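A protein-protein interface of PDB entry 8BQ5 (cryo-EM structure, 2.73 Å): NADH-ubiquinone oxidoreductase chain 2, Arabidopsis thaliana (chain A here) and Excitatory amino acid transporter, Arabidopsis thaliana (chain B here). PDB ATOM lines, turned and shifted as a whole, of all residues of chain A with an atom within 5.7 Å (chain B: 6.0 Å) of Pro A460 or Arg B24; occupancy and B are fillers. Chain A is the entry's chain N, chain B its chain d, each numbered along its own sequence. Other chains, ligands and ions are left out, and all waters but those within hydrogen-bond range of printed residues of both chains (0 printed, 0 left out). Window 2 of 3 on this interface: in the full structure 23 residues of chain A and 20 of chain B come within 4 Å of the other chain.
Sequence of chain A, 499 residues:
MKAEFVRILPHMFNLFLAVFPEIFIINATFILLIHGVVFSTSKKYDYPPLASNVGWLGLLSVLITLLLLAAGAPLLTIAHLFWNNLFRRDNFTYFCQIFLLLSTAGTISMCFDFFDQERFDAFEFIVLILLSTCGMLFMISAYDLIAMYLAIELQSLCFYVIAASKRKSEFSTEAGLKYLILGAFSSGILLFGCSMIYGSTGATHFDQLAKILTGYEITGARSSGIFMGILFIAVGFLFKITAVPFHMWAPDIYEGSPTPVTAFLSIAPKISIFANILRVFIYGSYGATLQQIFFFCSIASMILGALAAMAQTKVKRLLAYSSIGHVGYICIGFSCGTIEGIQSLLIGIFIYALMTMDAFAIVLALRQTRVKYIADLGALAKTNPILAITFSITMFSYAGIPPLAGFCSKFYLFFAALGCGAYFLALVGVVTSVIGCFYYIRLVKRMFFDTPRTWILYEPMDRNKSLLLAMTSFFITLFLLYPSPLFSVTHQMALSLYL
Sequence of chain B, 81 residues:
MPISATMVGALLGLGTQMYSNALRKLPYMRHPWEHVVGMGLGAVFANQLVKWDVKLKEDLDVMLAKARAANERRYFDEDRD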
ATOM      1  N   ASP A 113      -3.113  21.478  27.882  1.00  0.00           N
ATOM      2  CA  ASP A 113      -3.602  22.033  26.623  1.00  0.00           C
ATOM      3  C   ASP A 113      -3.814  23.534  26.738  1.00  0.00           C
ATOM      4  O   ASP A 113      -3.554  24.284  25.789  1.00  0.00           O
ATOM      5  CB  ASP A 113      -4.901  21.343  26.211  1.00  0.00           C
ATOM      6  CG  ASP A 113      -4.695  20.331  25.108  1.00  0.00           C
ATOM      7  OD1 ASP A 113      -5.685  19.983  24.431  1.00  0.00           O
ATOM      8  OD2 ASP A 113      -3.544  19.889  24.914  1.00  0.00           O
ATOM      9  N   ALA A 365     -11.904  21.043  27.417  1.00  0.00           N
ATOM     10  CA  ALA A 365     -11.743  20.494  26.076  1.00  0.00           C
ATOM     11  C   ALA A 365     -12.410  21.381  25.034  1.00  0.00           C
ATOM     12  O   ALA A 365     -11.868  21.585  23.942  1.00  0.00           O
ATOM     13  CB  ALA A 365     -12.310  19.077  26.015  1.00  0.00           C
ATOM     14  N   ASN A 384     -19.375  15.216  17.294  1.00  0.00           N
ATOM     15  CA  ASN A 384     -18.608  14.384  18.212  1.00  0.00           C
ATOM     16  C   ASN A 384     -19.584  13.578  19.059  1.00  0.00           C
ATOM     17  O   ASN A 384     -19.893  13.964  20.193  1.00  0.00           O
ATOM     18  CB  ASN A 384     -17.685  15.232  19.090  1.00  0.00           C
ATOM     19  CG  ASN A 384     -16.586  14.413  19.744  1.00  0.00           C
ATOM     20  OD1 ASN A 384     -16.652  13.185  19.794  1.00  0.00           O
ATOM     21  ND2 ASN A 384     -15.558  15.092  20.236  1.00  0.00           N
ATOM     22  N   TYR A 458     -15.478  21.532  17.051  1.00  0.00           N
ATOM     23  CA  TYR A 458     -14.560  21.635  18.175  1.00  0.00           C
ATOM     24  C   TYR A 458     -13.324  20.772  17.954  1.00  0.00           C
ATOM     25  O   TYR A 458     -13.416  19.652  17.445  1.00  0.00           O
ATOM     26  CB  TYR A 458     -15.262  21.228  19.470  1.00  0.00           C
ATOM     27  CG  TYR A 458     -16.306  22.226  19.905  1.00  0.00           C
ATOM     28  CD1 TYR A 458     -15.966  23.310  20.699  1.00  0.00           C
ATOM     29  CD2 TYR A 458     -17.625  22.104  19.496  1.00  0.00           C
ATOM     30  CE1 TYR A 458     -16.910  24.233  21.089  1.00  0.00           C
ATOM     31  CE2 TYR A 458     -18.577  23.023  19.880  1.00  0.00           C
ATOM     32  CZ  TYR A 458     -18.213  24.085  20.677  1.00  0.00           C
ATOM     33  OH  TYR A 458     -19.156  25.005  21.065  1.00  0.00           O
ATOM     34  N   GLU A 459     -12.169  21.309  18.333  1.00  0.00           N
ATOM     35  CA  GLU A 459     -10.935  20.542  18.278  1.00  0.00           C
ATOM     36  C   GLU A 459     -10.984  19.393  19.284  1.00  0.00           C
ATOM     37  O   GLU A 459     -11.424  19.582  20.422  1.00  0.00           O
ATOM     38  CB  GLU A 459      -9.731  21.436  18.572  1.00  0.00           C
ATOM     39  CG  GLU A 459      -9.369  22.369  17.440  1.00  0.00           C
ATOM     40  CD  GLU A 459      -9.062  21.622  16.158  1.00  0.00           C
ATOM     41  OE1 GLU A 459      -9.841  21.752  15.192  1.00  0.00           O
ATOM     42  OE2 GLU A 459      -8.042  20.902  16.119  1.00  0.00           O
ATOM     43  N   PRO A 460     -10.535  18.199  18.896  1.00  0.00           N
ATOM     44  CA  PRO A 460     -10.527  17.070  19.835  1.00  0.00           C
ATOM     45  C   PRO A 460      -9.607  17.326  21.019  1.00  0.00           C
ATOM     46  O   PRO A 460      -8.597  18.023  20.914  1.00  0.00           O
ATOM     47  CB  PRO A 460     -10.028  15.898  18.981  1.00  0.00           C
ATOM     48  CG  PRO A 460      -9.316  16.534  17.832  1.00  0.00           C
ATOM     49  CD  PRO A 460     -10.024  17.824  17.567  1.00  0.00           C
ATOM     50  N   MET A 461      -9.971  16.746  22.160  1.00  0.00           N
ATOM     51  CA  MET A 461      -9.238  16.979  23.394  1.00  0.00           C
ATOM     52  C   MET A 461      -7.951  16.163  23.432  1.00  0.00           C
ATOM     53  O   MET A 461      -7.764  15.205  22.678  1.00  0.00           O
ATOM     54  CB  MET A 461     -10.092  16.632  24.611  1.00  0.00           C
ATOM     55  CG  MET A 461     -10.586  15.200  24.644  1.00  0.00           C
ATOM     56  SD  MET A 461     -11.656  14.906  26.059  1.00  0.00           S
ATOM     57  CE  MET A 461     -13.205  15.524  25.419  1.00  0.00           C
ATOM     58  N   ASP A 462      -7.060  16.557  24.336  1.00  0.00           N
ATOM     59  CA  ASP A 462      -5.804  15.854  24.523  1.00  0.00           C
ATOM     60  C   ASP A 462      -6.020  14.572  25.328  1.00  0.00           C
ATOM     61  O   ASP A 462      -7.120  14.278  25.803  1.00  0.00           O
ATOM     62  CB  ASP A 462      -4.773  16.764  25.197  1.00  0.00           C
ATOM     63  CG  ASP A 462      -5.198  17.227  26.585  1.00  0.00           C
ATOM     64  OD1 ASP A 462      -6.242  16.776  27.097  1.00  0.00           O
ATOM     65  OD2 ASP A 462      -4.468  18.052  27.175  1.00  0.00           O
ATOM     66  N   ARG A 463      -4.939  13.810  25.491  1.00  0.00           N
ATOM     67  CA  ARG A 463      -5.049  12.493  26.112  1.00  0.00           C
ATOM     68  C   ARG A 463      -5.387  12.592  27.596  1.00  0.00           C
ATOM     69  O   ARG A 463      -6.137  11.761  28.122  1.00  0.00           O
ATOM     70  CB  ARG A 463      -3.753  11.715  25.905  1.00  0.00           C
ATOM     71  CG  ARG A 463      -3.826  10.269  26.342  1.00  0.00           C
ATOM     72  CD  ARG A 463      -2.437   9.712  26.554  1.00  0.00           C
ATOM     73  NE  ARG A 463      -1.746   9.523  25.285  1.00  0.00           N
ATOM     74  CZ  ARG A 463      -1.762   8.401  24.582  1.00  0.00           C
ATOM     75  NH1 ARG A 463      -2.406   7.327  25.009  1.00  0.00           N
ATOM     76  NH2 ARG A 463      -1.114   8.354  23.423  1.00  0.00           N
ATOM     77  N   SER A 466      -9.092  13.183  28.090  1.00  0.00           N
ATOM     78  CA  SER A 466      -9.873  12.029  27.651  1.00  0.00           C
ATOM     79  C   SER A 466      -9.792  10.888  28.656  1.00  0.00           C
ATOM     80  O   SER A 466     -10.803  10.244  28.952  1.00  0.00           O
ATOM     81  CB  SER A 466      -9.408  11.558  26.273  1.00  0.00           C
ATOM     82  OG  SER A 466      -8.037  11.209  26.287  1.00  0.00           O
ATOM     83  N   GLN B  17      -9.438   2.802  27.695  1.00  0.00           N
ATOM     84  CA  GLN B  17      -8.511   3.115  26.579  1.00  0.00           C
ATOM     85  C   GLN B  17      -9.305   3.371  25.288  1.00  0.00           C
ATOM     86  O   GLN B  17      -9.023   4.375  24.627  1.00  0.00           O
ATOM     87  CB  GLN B  17      -7.480   1.995  26.424  1.00  0.00           C
ATOM     88  CG  GLN B  17      -6.541   2.175  25.239  1.00  0.00           C
ATOM     89  CD  GLN B  17      -5.766   3.472  25.222  1.00  0.00           C
ATOM     90  OE1 GLN B  17      -5.434   4.044  26.257  1.00  0.00           O
ATOM     91  NE2 GLN B  17      -5.454   3.937  24.025  1.00  0.00           N
ATOM     92  N   TYR B  19     -12.523   4.187  25.089  1.00  0.00           N
ATOM     93  CA  TYR B  19     -13.332   5.404  25.362  1.00  0.00           C
ATOM     94  C   TYR B  19     -12.436   6.631  25.177  1.00  0.00           C
ATOM     95  O   TYR B  19     -12.863   7.580  24.522  1.00  0.00           O
ATOM     96  CB  TYR B  19     -13.912   5.288  26.774  1.00  0.00           C
ATOM     97  CG  TYR B  19     -15.082   6.159  27.148  1.00  0.00           C
ATOM     98  CD1 TYR B  19     -15.565   7.145  26.306  1.00  0.00           C
ATOM     99  CD2 TYR B  19     -15.706   5.988  28.371  1.00  0.00           C
ATOM    100  CE1 TYR B  19     -16.636   7.939  26.672  1.00  0.00           C
ATOM    101  CE2 TYR B  19     -16.783   6.769  28.751  1.00  0.00           C
ATOM    102  CZ  TYR B  19     -17.248   7.751  27.898  1.00  0.00           C
ATOM    103  OH  TYR B  19     -18.311   8.520  28.266  1.00  0.00           O
ATOM    104  N   SER B  20     -11.217   6.590  25.713  1.00  0.00           N
ATOM    105  CA  SER B  20     -10.235   7.698  25.558  1.00  0.00           C
ATOM    106  C   SER B  20      -9.884   7.902  24.079  1.00  0.00           C
ATOM    107  O   SER B  20      -9.860   9.055  23.655  1.00  0.00           O
ATOM    108  CB  SER B  20      -9.011   7.427  26.386  1.00  0.00           C
ATOM    109  OG  SER B  20      -7.999   8.387  26.137  1.00  0.00           O
ATOM    110  N   ASN B  21      -9.675   6.821  23.327  1.00  0.00           N
ATOM    111  CA  ASN B  21      -9.395   6.922  21.869  1.00  0.00           C
ATOM    112  C   ASN B  21     -10.597   7.538  21.155  1.00  0.00           C
ATOM    113  O   ASN B  21     -10.378   8.415  20.317  1.00  0.00           O
ATOM    114  CB  ASN B  21      -9.061   5.562  21.257  1.00  0.00           C
ATOM    115  CG  ASN B  21      -7.601   5.191  21.397  1.00  0.00           C
ATOM    116  OD1 ASN B  21      -6.751   6.053  21.586  1.00  0.00           O
ATOM    117  ND2 ASN B  21      -7.300   3.910  21.295  1.00  0.00           N
ATOM    118  N   ALA B  22     -11.811   7.101  21.492  1.00  0.00           N
ATOM    119  CA  ALA B  22     -13.041   7.603  20.839  1.00  0.00           C
ATOM    120  C   ALA B  22     -13.285   9.084  21.172  1.00  0.00           C
ATOM    121  O   ALA B  22     -13.698   9.815  20.260  1.00  0.00           O
ATOM    122  CB  ALA B  22     -14.209   6.740  21.248  1.00  0.00           C
ATOM    123  N   LEU B  23     -13.031   9.508  22.414  1.00  0.00           N
ATOM    124  CA  LEU B  23     -13.179  10.936  22.800  1.00  0.00           C
ATOM    125  C   LEU B  23     -12.228  11.807  21.977  1.00  0.00           C
ATOM    126  O   LEU B  23     -12.569  12.971  21.743  1.00  0.00           O
ATOM    127  CB  LEU B  23     -12.927  11.100  24.304  1.00  0.00           C
ATOM    128  CG  LEU B  23     -14.063  10.635  25.211  1.00  0.00           C
ATOM    129  CD1 LEU B  23     -13.595  10.509  26.652  1.00  0.00           C
ATOM    130  CD2 LEU B  23     -15.259  11.567  25.109  1.00  0.00           C
ATOM    131  N   ARG B  24     -11.083  11.263  21.562  1.00  0.00           N
ATOM    132  CA  ARG B  24     -10.143  12.019  20.749  1.00  0.00           C
ATOM    133  C   ARG B  24     -10.391  11.839  19.260  1.00  0.00           C
ATOM    134  O   ARG B  24      -9.589  12.313  18.450  1.00  0.00           O
ATOM    135  CB  ARG B  24      -8.712  11.612  21.096  1.00  0.00           C
ATOM    136  CG  ARG B  24      -8.418  11.683  22.577  1.00  0.00           C
ATOM    137  CD  ARG B  24      -7.169  10.912  22.935  1.00  0.00           C
ATOM    138  NE  ARG B  24      -5.982  11.506  22.336  1.00  0.00           N
ATOM    139  CZ  ARG B  24      -4.847  10.856  22.121  1.00  0.00           C
ATOM    140  NH1 ARG B  24      -4.703   9.586  22.457  1.00  0.00           N
ATOM    141  NH2 ARG B  24      -3.828  11.501  21.563  1.00  0.00           N
ATOM    142  N   LYS B  25     -11.479  11.159  18.894  1.00  0.00           N
ATOM    143  CA  LYS B  25     -11.831  10.872  17.504  1.00  0.00           C
ATOM    144  C   LYS B  25     -10.774  10.023  16.810  1.00  0.00           C
ATOM    145  O   LYS B  25     -10.571  10.129  15.599  1.00  0.00           O
ATOM    146  CB  LYS B  25     -12.088  12.156  16.713  1.00  0.00           C
ATOM    147  CG  LYS B  25     -13.336  12.885  17.143  1.00  0.00           C
ATOM    148  CD  LYS B  25     -14.428  12.712  16.114  1.00  0.00           C
ATOM    149  CE  LYS B  25     -15.056  14.037  15.763  1.00  0.00           C
ATOM    150  NZ  LYS B  25     -15.900  13.931  14.543  1.00  0.00           N
ATOM    151  N   LEU B  26     -10.104   9.177  17.563  1.00  0.00           N
ATOM    152  CA  LEU B  26      -9.145   8.244  17.003  1.00  0.00           C
ATOM    153  C   LEU B  26      -9.782   6.879  16.805  1.00  0.00           C
ATOM    154  O   LEU B  26     -10.839   6.585  17.369  1.00  0.00           O
ATOM    155  CB  LEU B  26      -7.928   8.110  17.920  1.00  0.00           C
ATOM    156  CG  LEU B  26      -7.053   9.347  18.100  1.00  0.00           C
ATOM    157  CD1 LEU B  26      -6.060   9.112  19.218  1.00  0.00           C
ATOM    158  CD2 LEU B  26      -6.341   9.686  16.807  1.00  0.00           C
ATOM    159  N   GLU B  34      -1.178   0.162  24.508  1.00  0.00           N
ATOM    160  CA  GLU B  34      -1.852   0.917  25.555  1.00  0.00           C
ATOM    161  C   GLU B  34      -3.103   0.200  26.043  1.00  0.00           C
ATOM    162  O   GLU B  34      -3.455   0.314  27.219  1.00  0.00           O
ATOM    163  CB  GLU B  34      -2.196   2.315  25.056  1.00  0.00           C
ATOM    164  CG  GLU B  34      -0.985   3.102  24.620  1.00  0.00           C
ATOM    165  CD  GLU B  34      -1.346   4.453  24.054  1.00  0.00           C
ATOM    166  OE1 GLU B  34      -2.551   4.734  23.895  1.00  0.00           O
ATOM    167  OE2 GLU B  34      -0.420   5.231  23.757  1.00  0.00           O
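The guanidinium group of Arg A463 lies within salt-bridge range of the side-chain carboxylate of Glu B34 (2.8 Å). OG of Ser B20 is in hydrogen-bond range of OG of Ser A466 (2.8 Å).
Of chain B, only Arg B24 comes within 4 Å of Pro A460. Arg B24 touches four residues of chain A. Printed residues of chain B within 4 Å of Ser A466: Ser B20 (2.8 Å), Leu B23 (3.6 Å) and Arg B24 (3.5 Å). Of the printed residues of chain B, Asn A384 touches Leu B23 (3.96 Å). Ala A365 touches none of the printed residues of chain B. The nearest residue of chain B that does not touch Pro A460 is Leu B23 (4.8 Å). The nearest printed residue of chain B that does not touch Asn A384 is Lys B25 (4.3 Å).
The side-chain amide nitrogen (NE2) of Gln B17 sits at hydrogen-bond distance from the side-chain carboxylate (OE1) of Glu B34, 3.0 Å away. The side-chain sulfur of Met A461 lies within hydrogen-bond range of the backbone NH of Ser A466 (3.7 Å). The backbone carbonyl oxygen of Asp A462 lies within hydrogen-bond range of the side-chain hydroxyl of Ser A466 (3.2 Å). O of Arg A463 lies within hydrogen-bond range of OG of Ser A466 (2.7 Å).
Leu B23 touches Asn A384 (O to ND2, 3.96 Å). Pro A460 touches Arg B24 (CB to O, 3.7 Å). Arg B24 touches Met A461. Arg B24 touches Arg A463 (NH1 to CZ, 3.8 Å). Ser A466 touches Leu B23 (O to CD1, 3.6 Å). OG of Ser A466 touches CD of Arg B24 (3.5 Å).
Of the 10 printed residues of chain B, 4 touch a printed residue of chain A. Hydrophobic or aromatic side chains of chain B within 4 Å of the printed part of chain A: Leu B23. Hydrophobic or aromatic side chains of chain A within 4 Å of the printed part of chain B: Pro A460.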
